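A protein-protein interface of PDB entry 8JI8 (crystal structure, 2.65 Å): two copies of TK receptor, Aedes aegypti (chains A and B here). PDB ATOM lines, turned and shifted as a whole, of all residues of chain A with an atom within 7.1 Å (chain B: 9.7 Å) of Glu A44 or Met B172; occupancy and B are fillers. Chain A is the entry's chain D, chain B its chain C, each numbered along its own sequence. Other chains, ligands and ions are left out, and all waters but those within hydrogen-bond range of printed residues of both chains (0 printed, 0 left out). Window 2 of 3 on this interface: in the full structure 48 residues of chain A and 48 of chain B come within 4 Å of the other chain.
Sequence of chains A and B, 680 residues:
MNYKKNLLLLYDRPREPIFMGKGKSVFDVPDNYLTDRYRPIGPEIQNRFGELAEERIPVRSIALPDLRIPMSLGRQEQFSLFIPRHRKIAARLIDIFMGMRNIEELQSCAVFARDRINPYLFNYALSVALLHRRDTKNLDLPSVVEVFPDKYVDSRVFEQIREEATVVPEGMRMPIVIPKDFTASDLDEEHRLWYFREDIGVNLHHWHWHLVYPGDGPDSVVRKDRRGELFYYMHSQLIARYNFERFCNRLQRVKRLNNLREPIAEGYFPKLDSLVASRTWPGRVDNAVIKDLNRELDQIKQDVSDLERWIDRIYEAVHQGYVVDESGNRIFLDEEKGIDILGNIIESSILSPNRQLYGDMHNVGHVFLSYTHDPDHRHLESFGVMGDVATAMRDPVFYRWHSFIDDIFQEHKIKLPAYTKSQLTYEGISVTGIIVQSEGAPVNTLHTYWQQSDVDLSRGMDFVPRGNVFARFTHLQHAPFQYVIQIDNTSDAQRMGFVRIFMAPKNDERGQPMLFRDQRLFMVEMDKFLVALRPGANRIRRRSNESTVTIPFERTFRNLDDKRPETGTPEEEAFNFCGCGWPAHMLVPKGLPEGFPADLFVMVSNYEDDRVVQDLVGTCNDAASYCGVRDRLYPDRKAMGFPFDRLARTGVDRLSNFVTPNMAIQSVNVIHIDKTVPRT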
ATOM      1  N   ARG A  37     -11.640  -9.179 -29.201  1.00  0.00           N
ATOM      2  CA  ARG A  37     -11.110  -8.996 -27.856  1.00  0.00           C
ATOM      3  C   ARG A  37     -10.595  -7.562 -27.679  1.00  0.00           C
ATOM      4  O   ARG A  37     -10.794  -6.971 -26.622  1.00  0.00           O
ATOM      5  CB  ARG A  37     -10.049 -10.065 -27.551  1.00  0.00           C
ATOM      6  CG  ARG A  37      -9.105  -9.769 -26.385  1.00  0.00           C
ATOM      7  CD  ARG A  37      -9.760  -9.653 -25.012  1.00  0.00           C
ATOM      8  NE  ARG A  37      -8.864  -9.281 -23.907  1.00  0.00           N
ATOM      9  CZ  ARG A  37      -9.107  -8.337 -22.993  1.00  0.00           C
ATOM     10  NH1 ARG A  37      -8.462  -8.343 -21.844  1.00  0.00           N
ATOM     11  NH2 ARG A  37     -10.061  -7.446 -23.172  1.00  0.00           N
ATOM     12  N   ARG A  39     -11.025  -4.645 -29.768  1.00  0.00           N
ATOM     13  CA  ARG A  39     -11.729  -3.465 -30.249  1.00  0.00           C
ATOM     14  C   ARG A  39     -12.117  -2.598 -29.046  1.00  0.00           C
ATOM     15  O   ARG A  39     -11.754  -1.420 -28.994  1.00  0.00           O
ATOM     16  CB  ARG A  39     -12.934  -3.854 -31.112  1.00  0.00           C
ATOM     17  CG  ARG A  39     -13.247  -2.872 -32.234  1.00  0.00           C
ATOM     18  CD  ARG A  39     -14.314  -3.390 -33.200  1.00  0.00           C
ATOM     19  NE  ARG A  39     -13.924  -4.609 -33.914  1.00  0.00           N
ATOM     20  CZ  ARG A  39     -14.439  -5.828 -33.728  1.00  0.00           C
ATOM     21  NH1 ARG A  39     -15.384  -6.038 -32.830  1.00  0.00           N
ATOM     22  NH2 ARG A  39     -13.999  -6.852 -34.443  1.00  0.00           N
ATOM     23  N   PRO A  40     -12.789  -3.161 -28.010  1.00  0.00           N
ATOM     24  CA  PRO A  40     -13.212  -2.387 -26.837  1.00  0.00           C
ATOM     25  C   PRO A  40     -12.138  -1.573 -26.106  1.00  0.00           C
ATOM     26  O   PRO A  40     -12.419  -0.481 -25.618  1.00  0.00           O
ATOM     27  CB  PRO A  40     -13.730  -3.458 -25.863  1.00  0.00           C
ATOM     28  CG  PRO A  40     -14.121  -4.628 -26.742  1.00  0.00           C
ATOM     29  CD  PRO A  40     -13.143  -4.585 -27.892  1.00  0.00           C
ATOM     30  N   ILE A  41     -10.921  -2.122 -26.007  1.00  0.00           N
ATOM     31  CA  ILE A  41      -9.791  -1.450 -25.383  1.00  0.00           C
ATOM     32  C   ILE A  41      -8.862  -0.907 -26.467  1.00  0.00           C
ATOM     33  O   ILE A  41      -7.680  -0.702 -26.217  1.00  0.00           O
ATOM     34  CB  ILE A  41      -9.053  -2.415 -24.431  1.00  0.00           C
ATOM     35  CG1 ILE A  41      -8.217  -3.460 -25.178  1.00  0.00           C
ATOM     36  CG2 ILE A  41     -10.040  -3.077 -23.479  1.00  0.00           C
ATOM     37  CD1 ILE A  41      -7.362  -4.328 -24.283  1.00  0.00           C
ATOM     38  N   GLY A  42      -9.390  -0.684 -27.677  1.00  0.00           N
ATOM     39  CA  GLY A  42      -8.618  -0.085 -28.759  1.00  0.00           C
ATOM     40  C   GLY A  42      -7.883   1.190 -28.338  1.00  0.00           C
ATOM     41  O   GLY A  42      -6.669   1.297 -28.511  1.00  0.00           O
ATOM     42  N   PRO A  43      -8.594   2.194 -27.775  1.00  0.00           N
ATOM     43  CA  PRO A  43      -7.966   3.417 -27.259  1.00  0.00           C
ATOM     44  C   PRO A  43      -6.797   3.221 -26.289  1.00  0.00           C
ATOM     45  O   PRO A  43      -5.763   3.865 -26.437  1.00  0.00           O
ATOM     46  CB  PRO A  43      -9.118   4.122 -26.523  1.00  0.00           C
ATOM     47  CG  PRO A  43     -10.374   3.624 -27.215  1.00  0.00           C
ATOM     48  CD  PRO A  43     -10.057   2.199 -27.611  1.00  0.00           C
ATOM     49  N   GLU A  44      -6.946   2.314 -25.310  1.00  0.00           N
ATOM     50  CA  GLU A  44      -5.919   2.072 -24.297  1.00  0.00           C
ATOM     51  C   GLU A  44      -4.772   1.232 -24.862  1.00  0.00           C
ATOM     52  O   GLU A  44      -3.816   0.918 -24.150  1.00  0.00           O
ATOM     53  CB  GLU A  44      -6.498   1.351 -23.076  1.00  0.00           C
ATOM     54  CG  GLU A  44      -7.381   2.215 -22.192  1.00  0.00           C
ATOM     55  CD  GLU A  44      -8.659   2.716 -22.844  1.00  0.00           C
ATOM     56  OE1 GLU A  44      -8.860   3.952 -22.869  1.00  0.00           O
ATOM     57  OE2 GLU A  44      -9.447   1.876 -23.332  1.00  0.00           O
ATOM     58  N   ILE A  45      -4.892   0.856 -26.140  1.00  0.00           N
ATOM     59  CA  ILE A  45      -3.910   0.032 -26.823  1.00  0.00           C
ATOM     60  C   ILE A  45      -3.037   0.923 -27.709  1.00  0.00           C
ATOM     61  O   ILE A  45      -1.815   0.853 -27.617  1.00  0.00           O
ATOM     62  CB  ILE A  45      -4.624  -1.122 -27.571  1.00  0.00           C
ATOM     63  CG1 ILE A  45      -4.479  -2.463 -26.837  1.00  0.00           C
ATOM     64  CG2 ILE A  45      -4.155  -1.243 -29.015  1.00  0.00           C
ATOM     65  CD1 ILE A  45      -4.840  -2.435 -25.366  1.00  0.00           C
ATOM     66  N   GLN A  46      -3.648   1.795 -28.521  1.00  0.00           N
ATOM     67  CA  GLN A  46      -2.898   2.670 -29.415  1.00  0.00           C
ATOM     68  C   GLN A  46      -1.875   3.514 -28.642  1.00  0.00           C
ATOM     69  O   GLN A  46      -0.783   3.783 -29.146  1.00  0.00           O
ATOM     70  CB  GLN A  46      -3.855   3.574 -30.202  1.00  0.00           C
ATOM     71  CG  GLN A  46      -3.189   4.427 -31.283  1.00  0.00           C
ATOM     72  CD  GLN A  46      -2.511   3.630 -32.378  1.00  0.00           C
ATOM     73  OE1 GLN A  46      -3.127   2.818 -33.067  1.00  0.00           O
ATOM     74  NE2 GLN A  46      -1.224   3.867 -32.563  1.00  0.00           N
ATOM     75  N   ASN A  47      -2.235   3.948 -27.426  1.00  0.00           N
ATOM     76  CA  ASN A  47      -1.341   4.757 -26.605  1.00  0.00           C
ATOM     77  C   ASN A  47      -0.206   3.899 -26.055  1.00  0.00           C
ATOM     78  O   ASN A  47       0.887   4.404 -25.827  1.00  0.00           O
ATOM     79  CB  ASN A  47      -2.055   5.448 -25.432  1.00  0.00           C
ATOM     80  CG  ASN A  47      -2.726   6.756 -25.797  1.00  0.00           C
ATOM     81  OD1 ASN A  47      -2.612   7.229 -26.926  1.00  0.00           O
ATOM     82  ND2 ASN A  47      -3.426   7.351 -24.844  1.00  0.00           N
ATOM     83  N   ARG A  48      -0.472   2.610 -25.827  1.00  0.00           N
ATOM     84  CA  ARG A  48       0.427   1.772 -25.050  1.00  0.00           C
ATOM     85  C   ARG A  48       1.605   1.286 -25.906  1.00  0.00           C
ATOM     86  O   ARG A  48       2.598   0.836 -25.337  1.00  0.00           O
ATOM     87  CB  ARG A  48      -0.369   0.624 -24.410  1.00  0.00           C
ATOM     88  CG  ARG A  48       0.436  -0.250 -23.452  1.00  0.00           C
ATOM     89  CD  ARG A  48      -0.381  -1.331 -22.755  1.00  0.00           C
ATOM     90  NE  ARG A  48       0.447  -2.346 -22.106  1.00  0.00           N
ATOM     91  CZ  ARG A  48       0.483  -2.601 -20.795  1.00  0.00           C
ATOM     92  NH1 ARG A  48       1.078  -3.693 -20.344  1.00  0.00           N
ATOM     93  NH2 ARG A  48      -0.118  -1.800 -19.931  1.00  0.00           N
ATOM     94  N   PHE A  49       1.508   1.379 -27.251  1.00  0.00           N
ATOM     95  CA  PHE A  49       2.561   0.911 -28.159  1.00  0.00           C
ATOM     96  C   PHE A  49       2.850   1.947 -29.247  1.00  0.00           C
ATOM     97  O   PHE A  49       1.980   2.744 -29.616  1.00  0.00           O
ATOM     98  CB  PHE A  49       2.198  -0.425 -28.832  1.00  0.00           C
ATOM     99  CG  PHE A  49       1.942  -1.567 -27.878  1.00  0.00           C
ATOM    100  CD1 PHE A  49       2.984  -2.334 -27.369  1.00  0.00           C
ATOM    101  CD2 PHE A  49       0.655  -1.826 -27.427  1.00  0.00           C
ATOM    102  CE1 PHE A  49       2.736  -3.346 -26.452  1.00  0.00           C
ATOM    103  CE2 PHE A  49       0.407  -2.839 -26.510  1.00  0.00           C
ATOM    104  CZ  PHE A  49       1.450  -3.593 -26.021  1.00  0.00           C
ATOM    105  N   GLU B 164      -2.135 -11.821 -22.696  1.00  0.00           N
ATOM    106  CA  GLU B 164      -2.990 -11.006 -21.858  1.00  0.00           C
ATOM    107  C   GLU B 164      -2.135 -10.083 -20.990  1.00  0.00           C
ATOM    108  O   GLU B 164      -2.346  -8.874 -21.002  1.00  0.00           O
ATOM    109  CB  GLU B 164      -3.885 -11.913 -21.017  1.00  0.00           C
ATOM    110  CG  GLU B 164      -4.938 -11.159 -20.217  1.00  0.00           C
ATOM    111  CD  GLU B 164      -6.120 -10.629 -21.010  1.00  0.00           C
ATOM    112  OE1 GLU B 164      -6.028 -10.578 -22.267  1.00  0.00           O
ATOM    113  OE2 GLU B 164      -7.145 -10.288 -20.365  1.00  0.00           O
ATOM    114  N   ALA B 165      -1.142 -10.665 -20.294  1.00  0.00           N
ATOM    115  CA  ALA B 165      -0.263  -9.955 -19.366  1.00  0.00           C
ATOM    116  C   ALA B 165       0.662  -8.946 -20.061  1.00  0.00           C
ATOM    117  O   ALA B 165       1.130  -8.021 -19.399  1.00  0.00           O
ATOM    118  CB  ALA B 165       0.548 -10.952 -18.573  1.00  0.00           C
ATOM    119  N   THR B 166       0.950  -9.120 -21.365  1.00  0.00           N
ATOM    120  CA  THR B 166       1.867  -8.240 -22.083  1.00  0.00           C
ATOM    121  C   THR B 166       1.125  -7.075 -22.733  1.00  0.00           C
ATOM    122  O   THR B 166       1.642  -5.961 -22.813  1.00  0.00           O
ATOM    123  CB  THR B 166       2.633  -8.990 -23.180  1.00  0.00           C
ATOM    124  OG1 THR B 166       3.445  -9.975 -22.548  1.00  0.00           O
ATOM    125  CG2 THR B 166       3.499  -8.084 -24.033  1.00  0.00           C
ATOM    126  N   VAL B 167      -0.076  -7.362 -23.239  1.00  0.00           N
ATOM    127  CA  VAL B 167      -0.796  -6.426 -24.084  1.00  0.00           C
ATOM    128  C   VAL B 167      -1.701  -5.568 -23.207  1.00  0.00           C
ATOM    129  O   VAL B 167      -1.704  -4.352 -23.328  1.00  0.00           O
ATOM    130  CB  VAL B 167      -1.574  -7.194 -25.172  1.00  0.00           C
ATOM    131  CG1 VAL B 167      -2.399  -6.280 -26.063  1.00  0.00           C
ATOM    132  CG2 VAL B 167      -0.634  -8.051 -26.007  1.00  0.00           C
ATOM    133  N   VAL B 168      -2.436  -6.215 -22.302  1.00  0.00           N
ATOM    134  CA  VAL B 168      -3.497  -5.559 -21.554  1.00  0.00           C
ATOM    135  C   VAL B 168      -2.935  -4.953 -20.262  1.00  0.00           C
ATOM    136  O   VAL B 168      -2.118  -5.574 -19.583  1.00  0.00           O
ATOM    137  CB  VAL B 168      -4.645  -6.554 -21.270  1.00  0.00           C
ATOM    138  CG1 VAL B 168      -5.812  -5.896 -20.556  1.00  0.00           C
ATOM    139  CG2 VAL B 168      -5.110  -7.254 -22.543  1.00  0.00           C
ATOM    140  N   PRO B 169      -3.365  -3.725 -19.870  1.00  0.00           N
ATOM    141  CA  PRO B 169      -3.001  -3.150 -18.574  1.00  0.00           C
ATOM    142  C   PRO B 169      -3.743  -3.789 -17.397  1.00  0.00           C
ATOM    143  O   PRO B 169      -4.930  -4.119 -17.488  1.00  0.00           O
ATOM    144  CB  PRO B 169      -3.391  -1.664 -18.677  1.00  0.00           C
ATOM    145  CG  PRO B 169      -3.792  -1.440 -20.130  1.00  0.00           C
ATOM    146  CD  PRO B 169      -4.195  -2.799 -20.662  1.00  0.00           C
ATOM    147  N   GLU B 170      -3.018  -3.870 -16.275  1.00  0.00           N
ATOM    148  CA  GLU B 170      -3.386  -4.612 -15.077  1.00  0.00           C
ATOM    149  C   GLU B 170      -4.857  -4.460 -14.681  1.00  0.00           C
ATOM    150  O   GLU B 170      -5.491  -5.449 -14.301  1.00  0.00           O
ATOM    151  CB  GLU B 170      -2.459  -4.190 -13.937  1.00  0.00           C
ATOM    152  CG  GLU B 170      -1.111  -4.863 -14.053  1.00  0.00           C
ATOM    153  CD  GLU B 170      -0.028  -4.401 -13.096  1.00  0.00           C
ATOM    154  OE1 GLU B 170       1.087  -4.069 -13.591  1.00  0.00           O
ATOM    155  OE2 GLU B 170      -0.287  -4.408 -11.862  1.00  0.00           O
ATOM    156  N   GLY B 171      -5.397  -3.239 -14.742  1.00  0.00           N
ATOM    157  CA  GLY B 171      -6.767  -3.004 -14.315  1.00  0.00           C
ATOM    158  C   GLY B 171      -7.816  -3.644 -15.227  1.00  0.00           C
ATOM    159  O   GLY B 171      -8.984  -3.708 -14.849  1.00  0.00           O
ATOM    160  N   MET B 172      -7.400  -4.133 -16.409  1.00  0.00           N
ATOM    161  CA  MET B 172      -8.328  -4.415 -17.495  1.00  0.00           C
ATOM    162  C   MET B 172      -8.272  -5.873 -17.935  1.00  0.00           C
ATOM    163  O   MET B 172      -9.019  -6.235 -18.845  1.00  0.00           O
ATOM    164  CB  MET B 172      -8.011  -3.531 -18.706  1.00  0.00           C
ATOM    165  CG  MET B 172      -8.892  -2.298 -18.813  1.00  0.00           C
ATOM    166  SD  MET B 172      -8.040  -0.927 -19.640  1.00  0.00           S
ATOM    167  CE  MET B 172      -7.932  -1.575 -21.304  1.00  0.00           C
ATOM    168  N   ARG B 173      -7.418  -6.692 -17.290  1.00  0.00           N
ATOM    169  CA  ARG B 173      -7.179  -8.076 -17.712  1.00  0.00           C
ATOM    170  C   ARG B 173      -8.312  -8.988 -17.241  1.00  0.00           C
ATOM    171  O   ARG B 173      -8.687  -8.973 -16.068  1.00  0.00           O
ATOM    172  CB  ARG B 173      -5.852  -8.624 -17.167  1.00  0.00           C
ATOM    173  CG  ARG B 173      -4.617  -7.959 -17.756  1.00  0.00           C
ATOM    174  CD  ARG B 173      -3.320  -8.195 -17.005  1.00  0.00           C
ATOM    175  NE  ARG B 173      -2.316  -7.280 -17.531  1.00  0.00           N
ATOM    176  CZ  ARG B 173      -1.113  -7.084 -17.003  1.00  0.00           C
ATOM    177  NH1 ARG B 173      -0.701  -7.821 -15.982  1.00  0.00           N
ATOM    178  NH2 ARG B 173      -0.315  -6.170 -17.528  1.00  0.00           N
ATOM    179  N   MET B 174      -8.837  -9.807 -18.162  1.00  0.00           N
ATOM    180  CA  MET B 174      -9.974 -10.643 -17.829  1.00  0.00           C
ATOM    181  C   MET B 174      -9.471 -12.051 -17.514  1.00  0.00           C
ATOM    182  O   MET B 174      -8.428 -12.468 -18.013  1.00  0.00           O
ATOM    183  CB  MET B 174     -11.017 -10.628 -18.954  1.00  0.00           C
ATOM    184  CG  MET B 174     -12.009  -9.426 -18.869  1.00  0.00           C
ATOM    185  SD  MET B 174     -12.809  -9.108 -17.218  1.00  0.00           S
ATOM    186  CE  MET B 174     -12.102  -7.528 -16.736  1.00  0.00           C
ATOM    187  N   PRO B 175     -10.139 -12.793 -16.601  1.00  0.00           N
ATOM    188  CA  PRO B 175      -9.650 -14.111 -16.181  1.00  0.00           C
ATOM    189  C   PRO B 175      -9.667 -15.144 -17.304  1.00  0.00           C
ATOM    190  O   PRO B 175     -10.516 -15.095 -18.186  1.00  0.00           O
ATOM    191  CB  PRO B 175     -10.611 -14.548 -15.059  1.00  0.00           C
ATOM    192  CG  PRO B 175     -11.354 -13.273 -14.651  1.00  0.00           C
ATOM    193  CD  PRO B 175     -11.371 -12.400 -15.893  1.00  0.00           C
ATOM    194  N   GLY B 467       1.380  -8.729 -12.167  1.00  0.00           N
ATOM    195  CA  GLY B 467      -0.065  -8.638 -12.273  1.00  0.00           C
ATOM    196  C   GLY B 467      -0.760  -9.924 -11.829  1.00  0.00           C
ATOM    197  O   GLY B 467      -0.267 -11.025 -12.056  1.00  0.00           O
ATOM    198  N   ASN B 468      -1.906  -9.753 -11.165  1.00  0.00           N
ATOM    199  CA  ASN B 468      -2.828 -10.839 -10.912  1.00  0.00           C
ATOM    200  C   ASN B 468      -3.067 -11.577 -12.213  1.00  0.00           C
ATOM    201  O   ASN B 468      -3.147 -10.954 -13.264  1.00  0.00           O
ATOM    202  CB  ASN B 468      -4.164 -10.323 -10.387  1.00  0.00           C
ATOM    203  CG  ASN B 468      -4.063  -9.816  -8.970  1.00  0.00           C
ATOM    204  OD1 ASN B 468      -3.121 -10.141  -8.250  1.00  0.00           O
ATOM    205  ND2 ASN B 468      -5.052  -9.044  -8.557  1.00  0.00           N
ATOM    206  N   PHE B 470      -5.875 -14.361 -12.874  1.00  0.00           N
ATOM    207  CA  PHE B 470      -6.943 -15.182 -12.326  1.00  0.00           C
ATOM    208  C   PHE B 470      -7.331 -16.244 -13.351  1.00  0.00           C
ATOM    209  O   PHE B 470      -7.564 -15.922 -14.508  1.00  0.00           O
ATOM    210  CB  PHE B 470      -8.112 -14.301 -11.882  1.00  0.00           C
ATOM    211  CG  PHE B 470      -7.813 -13.444 -10.679  1.00  0.00           C
ATOM    212  CD1 PHE B 470      -7.343 -14.014  -9.501  1.00  0.00           C
ATOM    213  CD2 PHE B 470      -8.012 -12.076 -10.713  1.00  0.00           C
ATOM    214  CE1 PHE B 470      -7.060 -13.232  -8.392  1.00  0.00           C
ATOM    215  CE2 PHE B 470      -7.735 -11.295  -9.602  1.00  0.00           C
ATOM    216  CZ  PHE B 470      -7.255 -11.870  -8.446  1.00  0.00           C
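The guanidinium group of Arg A48 is in hydrogen-bond range of the backbone carbonyl oxygen of Val B167, at 3.2 Å.
OE2 of Glu B164 is in salt-bridge range of NH1 of Arg A37, at 2.8 Å.
O of Thr B166 lies within hydrogen-bond range of NH1 of Arg A48, at 3.4 Å.
OE2 of Glu B164 sits at hydrogen-bond distance from N of Met B174 (2.8 Å).
The backbone carbonyl oxygen (O) of Val B168 lies within hydrogen-bond range of the guanidinium group (NE) of Arg B173, at 2.7 Å.
Val B168 touches Arg A37.
Arg A37 touches Met B172 (NH1 to O, 3.7 Å).
Met B174 touches Arg A37.
Ile A41 touches Met B172.
Glu A44 touches Met B172 (CB to CE, 3.7 Å).
Arg A48 touches Val B168 (NH1 to O, 3.8 Å).
Arg A48 touches Pro B169.
O of Thr B166 touches CZ of Phe A49 (3.99 Å).
Of the printed residues of chain B, Arg A37 touches Glu B164 (2.8 Å), Val B168 (3.6 Å), Met B172 (3.7 Å) and Met B174 (3.98 Å).
Ile A41 touches just one residue of chain B: Met B172.
No residue of chain B comes within 4 Å of Gly A42.
Glu A44 touches just one residue of chain B: Met B172 (3.7 Å).
No residue of chain B comes within 4 Å of Ile A45.
Of the printed residues of chain A, Glu B164 touches Arg A37.
Of the printed residues of chain A, Thr B166 touches Arg A48 (3.4 Å) and Phe A49 (3.99 Å).
Of the printed residues of chain A, Val B167 touches Arg A48 (3.2 Å).
Of the printed residues of chain A, Val B168 touches Arg A37 (3.6 Å) and Arg A48 (3.8 Å).
No residue of chain A comes within 4 Å of Gly B171.
Pro B175 touches none of the printed residues of chain A.
The nearest residue of chain A that does not touch Met B172 is Ile A45 (5.2 Å).
The nearest printed residue of chain A that does not touch Met B174 is Ile A41 (8.1 Å).
Hydrophobic or aromatic side chains of chain B within 4 Å of the printed part of chain A: Val B168, Pro B169 and Met B172.
Of the 12 printed residues of chain A, 5 touch a printed residue of chain B.
Hydrophobic or aromatic side chains of chain A that line the printed part of chain B: Ile A41 and Phe A49.
Along chain A the printed residues that touch a printed residue of chain B span positions 37 to 49.
No position is printed for both chains.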
